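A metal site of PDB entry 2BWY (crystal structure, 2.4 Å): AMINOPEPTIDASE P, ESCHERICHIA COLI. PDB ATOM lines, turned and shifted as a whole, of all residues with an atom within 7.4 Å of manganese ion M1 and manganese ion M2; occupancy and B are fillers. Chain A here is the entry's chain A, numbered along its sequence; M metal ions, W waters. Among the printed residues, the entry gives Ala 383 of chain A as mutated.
OH of Tyr 229 touches manganese ion M2, 3.6 Å away.
Thr 273 touches manganese ion M2 (OG1 to MN, 3.5 Å).
OD1 of Asp 271 lies close to OH of Tyr 229, at 2.8 Å.
The side-chain carboxylate (OD1) of Asp 260 sits close to the side-chain hydroxyl (OH) of Tyr 229, 2.8 Å away.
The side-chain carboxylate (OD2) of Asp 260 lies close to the guanidinium group (NH2) of Arg 404.
The backbone NH (N) of Asp 260 is in hydrogen-bond range of the backbone carbonyl oxygen (O) of Ile 232 (2.8 Å).
N of Thr 381 sits at hydrogen-bond distance from O of His 354.
OG1 of Thr 273 is in hydrogen-bond range of NE of Arg 404, 3.3 Å away.
The side-chain hydroxyl of Tyr 229 lies close to the backbone NH of Ala 261, at 3.2 Å.
The side-chain hydroxyl of Tyr 229 lies within hydrogen-bond range of the backbone NH of Gly 262, 3.3 Å away.
Within 4 Å of manganese ion M1: Asp 271, His 354 and Glu 406.
The nearest printed residue that does not touch manganese ion M1 is Thr 381 (4.1 Å).
The side-chain carboxylate (OE1) of Glu 406 is bound to manganese ion M2 (2.1 Å).
OD1 of Asp 271 binds manganese ion M2, 2.2 Å away.
OD1 of Asp 260 binds manganese ion M2 (2.2 Å).
Manganese ion M2 is bound by the side-chain carboxylate (OD2) of Asp 260 (2.6 Å).
Manganese ion M2 has four donor atoms within binding distance.
The side-chain carboxylate (OD2) of Asp 271 is bound to manganese ion M1 (2.2 Å).
NE2 of His 354 is bound to manganese ion M1 (2.2 Å).
OE2 of Glu 406 binds manganese ion M1 (2.4 Å).
Slightly farther from manganese ion M1 lies water W1 (2.7 Å).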
ATOM      1  N   TYR A 229      17.986   0.146 -27.053  1.00  0.00           N
ATOM      2  CA  TYR A 229      19.386   0.000 -27.465  1.00  0.00           C
ATOM      3  C   TYR A 229      19.520   0.456 -28.920  1.00  0.00           C
ATOM      4  O   TYR A 229      18.517   0.654 -29.614  1.00  0.00           O
ATOM      5  CB  TYR A 229      19.870  -1.455 -27.303  1.00  0.00           C
ATOM      6  CG  TYR A 229      18.998  -2.451 -27.986  1.00  0.00           C
ATOM      7  CD1 TYR A 229      17.866  -2.949 -27.363  1.00  0.00           C
ATOM      8  CD2 TYR A 229      19.280  -2.894 -29.273  1.00  0.00           C
ATOM      9  CE1 TYR A 229      17.047  -3.848 -27.992  1.00  0.00           C
ATOM     10  CE2 TYR A 229      18.464  -3.796 -29.915  1.00  0.00           C
ATOM     11  CZ  TYR A 229      17.353  -4.274 -29.254  1.00  0.00           C
ATOM     12  OH  TYR A 229      16.513  -5.164 -29.853  1.00  0.00           O
ATOM     13  N   ILE A 232      20.011  -2.355 -34.814  1.00  0.00           N
ATOM     14  CA  ILE A 232      20.835  -3.123 -35.727  1.00  0.00           C
ATOM     15  C   ILE A 232      20.046  -3.463 -36.983  1.00  0.00           C
ATOM     16  O   ILE A 232      18.969  -4.037 -36.913  1.00  0.00           O
ATOM     17  CB  ILE A 232      21.311  -4.440 -35.039  1.00  0.00           C
ATOM     18  CG1 ILE A 232      22.218  -4.113 -33.833  1.00  0.00           C
ATOM     19  CG2 ILE A 232      22.020  -5.377 -36.025  1.00  0.00           C
ATOM     20  CD1 ILE A 232      22.155  -5.131 -32.735  1.00  0.00           C
ATOM     21  N   HIS A 243      26.582  -6.810 -33.267  1.00  0.00           N
ATOM     22  CA  HIS A 243      26.040  -5.477 -32.928  1.00  0.00           C
ATOM     23  C   HIS A 243      26.469  -4.461 -34.010  1.00  0.00           C
ATOM     24  O   HIS A 243      27.151  -3.469 -33.734  1.00  0.00           O
ATOM     25  CB  HIS A 243      26.416  -5.067 -31.484  1.00  0.00           C
ATOM     26  CG  HIS A 243      25.913  -6.019 -30.416  1.00  0.00           C
ATOM     27  ND1 HIS A 243      26.588  -6.227 -29.219  1.00  0.00           N
ATOM     28  CD2 HIS A 243      24.819  -6.810 -30.358  1.00  0.00           C
ATOM     29  CE1 HIS A 243      25.920  -7.101 -28.484  1.00  0.00           C
ATOM     30  NE2 HIS A 243      24.844  -7.471 -29.155  1.00  0.00           N
ATOM     31  N   ILE A 259      17.329  -7.610 -38.608  1.00  0.00           N
ATOM     32  CA  ILE A 259      16.944  -6.430 -37.834  1.00  0.00           C
ATOM     33  C   ILE A 259      16.845  -6.775 -36.370  1.00  0.00           C
ATOM     34  O   ILE A 259      16.038  -7.609 -35.989  1.00  0.00           O
ATOM     35  CB  ILE A 259      15.609  -5.847 -38.286  1.00  0.00           C
ATOM     36  CG1 ILE A 259      15.655  -5.546 -39.781  1.00  0.00           C
ATOM     37  CG2 ILE A 259      15.309  -4.577 -37.501  1.00  0.00           C
ATOM     38  CD1 ILE A 259      14.493  -4.709 -40.245  1.00  0.00           C
ATOM     39  N   ASP A 260      17.674  -6.122 -35.551  1.00  0.00           N
ATOM     40  CA  ASP A 260      17.599  -6.258 -34.101  1.00  0.00           C
ATOM     41  C   ASP A 260      17.254  -4.894 -33.488  1.00  0.00           C
ATOM     42  O   ASP A 260      18.067  -3.965 -33.487  1.00  0.00           O
ATOM     43  CB  ASP A 260      18.928  -6.788 -33.537  1.00  0.00           C
ATOM     44  CG  ASP A 260      18.783  -7.374 -32.124  1.00  0.00           C
ATOM     45  OD1 ASP A 260      17.821  -7.045 -31.375  1.00  0.00           O
ATOM     46  OD2 ASP A 260      19.662  -8.181 -31.769  1.00  0.00           O
ATOM     47  N   ALA A 261      16.030  -4.799 -32.966  1.00  0.00           N
ATOM     48  CA  ALA A 261      15.518  -3.532 -32.474  1.00  0.00           C
ATOM     49  C   ALA A 261      14.462  -3.716 -31.397  1.00  0.00           C
ATOM     50  O   ALA A 261      13.674  -4.687 -31.388  1.00  0.00           O
ATOM     51  CB  ALA A 261      14.958  -2.723 -33.609  1.00  0.00           C
ATOM     52  N   GLY A 262      14.424  -2.748 -30.494  1.00  0.00           N
ATOM     53  CA  GLY A 262      13.595  -2.818 -29.302  1.00  0.00           C
ATOM     54  C   GLY A 262      13.267  -1.427 -28.835  1.00  0.00           C
ATOM     55  O   GLY A 262      14.111  -0.534 -28.922  1.00  0.00           O
ATOM     56  N   GLY A 270      11.708  -3.686 -24.952  1.00  0.00           N
ATOM     57  CA  GLY A 270      11.412  -4.717 -25.928  1.00  0.00           C
ATOM     58  C   GLY A 270      12.727  -5.113 -26.564  1.00  0.00           C
ATOM     59  O   GLY A 270      13.685  -4.320 -26.572  1.00  0.00           O
ATOM     60  N   ASP A 271      12.794  -6.326 -27.091  1.00  0.00           N
ATOM     61  CA  ASP A 271      14.003  -6.794 -27.771  1.00  0.00           C
ATOM     62  C   ASP A 271      13.688  -7.926 -28.754  1.00  0.00           C
ATOM     63  O   ASP A 271      13.606  -9.089 -28.368  1.00  0.00           O
ATOM     64  CB  ASP A 271      15.020  -7.246 -26.725  1.00  0.00           C
ATOM     65  CG  ASP A 271      16.306  -7.696 -27.324  1.00  0.00           C
ATOM     66  OD1 ASP A 271      16.431  -7.665 -28.574  1.00  0.00           O
ATOM     67  OD2 ASP A 271      17.190  -8.091 -26.537  1.00  0.00           O
ATOM     68  N   ILE A 272      13.535  -7.580 -30.024  1.00  0.00           N
ATOM     69  CA  ILE A 272      13.200  -8.562 -31.038  1.00  0.00           C
ATOM     70  C   ILE A 272      14.259  -8.551 -32.135  1.00  0.00           C
ATOM     71  O   ILE A 272      14.766  -7.482 -32.511  1.00  0.00           O
ATOM     72  CB  ILE A 272      11.847  -8.266 -31.688  1.00  0.00           C
ATOM     73  CG1 ILE A 272      10.719  -8.311 -30.660  1.00  0.00           C
ATOM     74  CG2 ILE A 272      11.553  -9.279 -32.834  1.00  0.00           C
ATOM     75  CD1 ILE A 272       9.353  -8.074 -31.267  1.00  0.00           C
ATOM     76  N   THR A 273      14.573  -9.746 -32.636  1.00  0.00           N
ATOM     77  CA  THR A 273      15.339  -9.891 -33.876  1.00  0.00           C
ATOM     78  C   THR A 273      14.518 -10.665 -34.871  1.00  0.00           C
ATOM     79  O   THR A 273      13.928 -11.692 -34.527  1.00  0.00           O
ATOM     80  CB  THR A 273      16.713 -10.595 -33.705  1.00  0.00           C
ATOM     81  OG1 THR A 273      17.420 -10.052 -32.577  1.00  0.00           O
ATOM     82  CG2 THR A 273      17.556 -10.391 -34.953  1.00  0.00           C
ATOM     83  N   LEU A 352      22.250 -17.873 -25.632  1.00  0.00           N
ATOM     84  CA  LEU A 352      20.877 -17.975 -26.163  1.00  0.00           C
ATOM     85  C   LEU A 352      19.918 -16.952 -25.557  1.00  0.00           C
ATOM     86  O   LEU A 352      19.001 -16.500 -26.224  1.00  0.00           O
ATOM     87  CB  LEU A 352      20.355 -19.388 -25.855  1.00  0.00           C
ATOM     88  CG  LEU A 352      18.973 -19.760 -26.390  1.00  0.00           C
ATOM     89  CD1 LEU A 352      18.990 -19.809 -27.887  1.00  0.00           C
ATOM     90  CD2 LEU A 352      18.584 -21.098 -25.821  1.00  0.00           C
ATOM     91  N   SER A 353      20.124 -16.607 -24.296  1.00  0.00           N
ATOM     92  CA  SER A 353      19.109 -15.914 -23.501  1.00  0.00           C
ATOM     93  C   SER A 353      19.714 -14.948 -22.491  1.00  0.00           C
ATOM     94  O   SER A 353      20.702 -15.283 -21.853  1.00  0.00           O
ATOM     95  CB  SER A 353      18.239 -16.941 -22.759  1.00  0.00           C
ATOM     96  OG  SER A 353      17.401 -17.664 -23.651  1.00  0.00           O
ATOM     97  N   HIS A 354      19.151 -13.741 -22.379  1.00  0.00           N
ATOM     98  CA  HIS A 354      19.494 -12.840 -21.281  1.00  0.00           C
ATOM     99  C   HIS A 354      18.228 -12.355 -20.604  1.00  0.00           C
ATOM    100  O   HIS A 354      17.161 -12.389 -21.199  1.00  0.00           O
ATOM    101  CB  HIS A 354      20.364 -11.658 -21.756  1.00  0.00           C
ATOM    102  CG  HIS A 354      19.762 -10.843 -22.858  1.00  0.00           C
ATOM    103  ND1 HIS A 354      18.844  -9.838 -22.644  1.00  0.00           N
ATOM    104  CD2 HIS A 354      19.970 -10.875 -24.207  1.00  0.00           C
ATOM    105  CE1 HIS A 354      18.500  -9.296 -23.804  1.00  0.00           C
ATOM    106  NE2 HIS A 354      19.168  -9.904 -24.761  1.00  0.00           N
ATOM    107  N   TRP A 355      18.353 -11.897 -19.357  1.00  0.00           N
ATOM    108  CA  TRP A 355      17.234 -11.313 -18.633  1.00  0.00           C
ATOM    109  C   TRP A 355      16.822 -10.020 -19.343  1.00  0.00           C
ATOM    110  O   TRP A 355      17.642  -9.347 -19.941  1.00  0.00           O
ATOM    111  CB  TRP A 355      17.597 -10.959 -17.177  1.00  0.00           C
ATOM    112  CG  TRP A 355      18.251 -12.013 -16.344  1.00  0.00           C
ATOM    113  CD1 TRP A 355      19.393 -11.869 -15.617  1.00  0.00           C
ATOM    114  CD2 TRP A 355      17.782 -13.353 -16.103  1.00  0.00           C
ATOM    115  NE1 TRP A 355      19.680 -13.031 -14.958  1.00  0.00           N
ATOM    116  CE2 TRP A 355      18.711 -13.961 -15.239  1.00  0.00           C
ATOM    117  CE3 TRP A 355      16.689 -14.101 -16.547  1.00  0.00           C
ATOM    118  CZ2 TRP A 355      18.583 -15.282 -14.813  1.00  0.00           C
ATOM    119  CZ3 TRP A 355      16.552 -15.391 -16.116  1.00  0.00           C
ATOM    120  CH2 TRP A 355      17.504 -15.979 -15.260  1.00  0.00           C
ATOM    121  N   LEU A 356      15.548  -9.678 -19.248  1.00  0.00           N
ATOM    122  CA  LEU A 356      15.004  -8.486 -19.866  1.00  0.00           C
ATOM    123  C   LEU A 356      14.151  -7.701 -18.852  1.00  0.00           C
ATOM    124  O   LEU A 356      13.374  -8.274 -18.097  1.00  0.00           O
ATOM    125  CB  LEU A 356      14.169  -8.910 -21.072  1.00  0.00           C
ATOM    126  CG  LEU A 356      13.609  -7.843 -22.007  1.00  0.00           C
ATOM    127  CD1 LEU A 356      14.689  -7.232 -22.870  1.00  0.00           C
ATOM    128  CD2 LEU A 356      12.503  -8.484 -22.845  1.00  0.00           C
ATOM    129  N   VAL A 360      17.846  -3.712 -21.259  1.00  0.00           N
ATOM    130  CA  VAL A 360      17.743  -4.782 -22.267  1.00  0.00           C
ATOM    131  C   VAL A 360      18.587  -6.014 -21.835  1.00  0.00           C
ATOM    132  O   VAL A 360      18.128  -7.158 -21.931  1.00  0.00           O
ATOM    133  CB  VAL A 360      18.092  -4.275 -23.698  1.00  0.00           C
ATOM    134  CG1 VAL A 360      19.514  -3.723 -23.767  1.00  0.00           C
ATOM    135  CG2 VAL A 360      17.924  -5.370 -24.737  1.00  0.00           C
ATOM    136  N   HIS A 361      19.791  -5.771 -21.332  1.00  0.00           N
ATOM    137  CA  HIS A 361      20.594  -6.795 -20.680  1.00  0.00           C
ATOM    138  C   HIS A 361      20.403  -6.617 -19.193  1.00  0.00           C
ATOM    139  O   HIS A 361      21.199  -5.932 -18.519  1.00  0.00           O
ATOM    140  CB  HIS A 361      22.067  -6.684 -21.061  1.00  0.00           C
ATOM    141  CG  HIS A 361      22.349  -6.936 -22.497  1.00  0.00           C
ATOM    142  ND1 HIS A 361      23.504  -6.534 -23.111  1.00  0.00           N
ATOM    143  CD2 HIS A 361      21.609  -7.542 -23.458  1.00  0.00           C
ATOM    144  CE1 HIS A 361      23.486  -6.894 -24.381  1.00  0.00           C
ATOM    145  NE2 HIS A 361      22.338  -7.506 -24.613  1.00  0.00           N
ATOM    146  N   THR A 381      15.058 -13.186 -23.018  1.00  0.00           N
ATOM    147  CA  THR A 381      15.087 -13.395 -24.454  1.00  0.00           C
ATOM    148  C   THR A 381      15.445 -14.823 -24.865  1.00  0.00           C
ATOM    149  O   THR A 381      16.071 -15.576 -24.105  1.00  0.00           O
ATOM    150  CB  THR A 381      16.033 -12.403 -25.137  1.00  0.00           C
ATOM    151  OG1 THR A 381      17.401 -12.705 -24.791  1.00  0.00           O
ATOM    152  CG2 THR A 381      15.661 -10.973 -24.722  1.00  0.00           C
ATOM    153  N   VAL A 382      14.996 -15.202 -26.071  1.00  0.00           N
ATOM    154  CA  VAL A 382      15.362 -16.464 -26.699  1.00  0.00           C
ATOM    155  C   VAL A 382      15.831 -16.060 -28.087  1.00  0.00           C
ATOM    156  O   VAL A 382      15.030 -15.603 -28.908  1.00  0.00           O
ATOM    157  CB  VAL A 382      14.174 -17.449 -26.763  1.00  0.00           C
ATOM    158  CG1 VAL A 382      14.663 -18.864 -27.139  1.00  0.00           C
ATOM    159  CG2 VAL A 382      13.441 -17.502 -25.416  1.00  0.00           C
ATOM    160  N   ALA A 383      17.129 -16.212 -28.349  1.00  0.00           N
ATOM    161  CA  ALA A 383      17.783 -15.585 -29.488  1.00  0.00           C
ATOM    162  C   ALA A 383      18.872 -16.454 -30.119  1.00  0.00           C
ATOM    163  O   ALA A 383      20.028 -16.071 -30.133  1.00  0.00           O
ATOM    164  CB  ALA A 383      18.386 -14.242 -29.056  1.00  0.00           C
ATOM    165  N   ARG A 404      19.550 -14.338 -37.181  1.00  0.00           N
ATOM    166  CA  ARG A 404      19.111 -14.450 -35.805  1.00  0.00           C
ATOM    167  C   ARG A 404      17.619 -14.224 -35.762  1.00  0.00           C
ATOM    168  O   ARG A 404      17.073 -13.444 -36.547  1.00  0.00           O
ATOM    169  CB  ARG A 404      19.829 -13.422 -34.912  1.00  0.00           C
ATOM    170  CG  ARG A 404      19.364 -13.389 -33.447  1.00  0.00           C
ATOM    171  CD  ARG A 404      20.337 -12.660 -32.522  1.00  0.00           C
ATOM    172  NE  ARG A 404      20.498 -11.206 -32.765  1.00  0.00           N
ATOM    173  CZ  ARG A 404      21.525 -10.632 -33.413  1.00  0.00           C
ATOM    174  NH1 ARG A 404      22.507 -11.343 -33.933  1.00  0.00           N
ATOM    175  NH2 ARG A 404      21.576  -9.318 -33.540  1.00  0.00           N
ATOM    176  N   GLU A 406      14.783 -13.715 -32.580  1.00  0.00           N
ATOM    177  CA  GLU A 406      14.739 -13.463 -31.145  1.00  0.00           C
ATOM    178  C   GLU A 406      13.357 -12.989 -30.728  1.00  0.00           C
ATOM    179  O   GLU A 406      12.774 -12.112 -31.353  1.00  0.00           O
ATOM    180  CB  GLU A 406      15.815 -12.433 -30.774  1.00  0.00           C
ATOM    181  CG  GLU A 406      15.699 -11.832 -29.407  1.00  0.00           C
ATOM    182  CD  GLU A 406      16.880 -10.985 -29.058  1.00  0.00           C
ATOM    183  OE1 GLU A 406      17.354 -10.236 -29.944  1.00  0.00           O
ATOM    184  OE2 GLU A 406      17.308 -11.041 -27.882  1.00  0.00           O
ATOM    185  N   ASP A 407      12.862 -13.614 -29.663  1.00  0.00           N
ATOM    186  CA  ASP A 407      11.578 -13.342 -29.031  1.00  0.00           C
ATOM    187  C   ASP A 407      11.826 -13.074 -27.535  1.00  0.00           C
ATOM    188  O   ASP A 407      12.864 -13.476 -27.003  1.00  0.00           O
ATOM    189  CB  ASP A 407      10.654 -14.549 -29.165  1.00  0.00           C
ATOM    190  CG  ASP A 407       9.784 -14.513 -30.431  1.00  0.00           C
ATOM    191  OD1 ASP A 407       9.577 -13.414 -31.000  1.00  0.00           O
ATOM    192  OD2 ASP A 407       9.270 -15.589 -30.830  1.00  0.00           O
ATOM    193  N   ASP A 408      10.861 -12.402 -26.903  1.00  0.00           N
ATOM    194  CA  ASP A 408      10.904 -12.064 -25.470  1.00  0.00           C
ATOM    195  C   ASP A 408       9.816 -12.869 -24.767  1.00  0.00           C
ATOM    196  O   ASP A 408       8.674 -12.931 -25.237  1.00  0.00           O
ATOM    197  CB  ASP A 408      10.658 -10.566 -25.238  1.00  0.00           C
ATOM    198  CG  ASP A 408      11.563  -9.662 -26.073  1.00  0.00           C
ATOM    199  OD1 ASP A 408      12.704 -10.063 -26.412  1.00  0.00           O
ATOM    200  OD2 ASP A 408      11.138  -8.545 -26.393  1.00  0.00           O
HETATM  201 MN    MN M   1      18.862  -9.485 -26.933  1.00  0.00          MN
HETATM  202 MN    MN M   2      18.163  -8.331 -29.674  1.00  0.00          MN
HETATM  203  O   HOH W   1      20.561  -7.507 -27.766  1.00  0.00           O
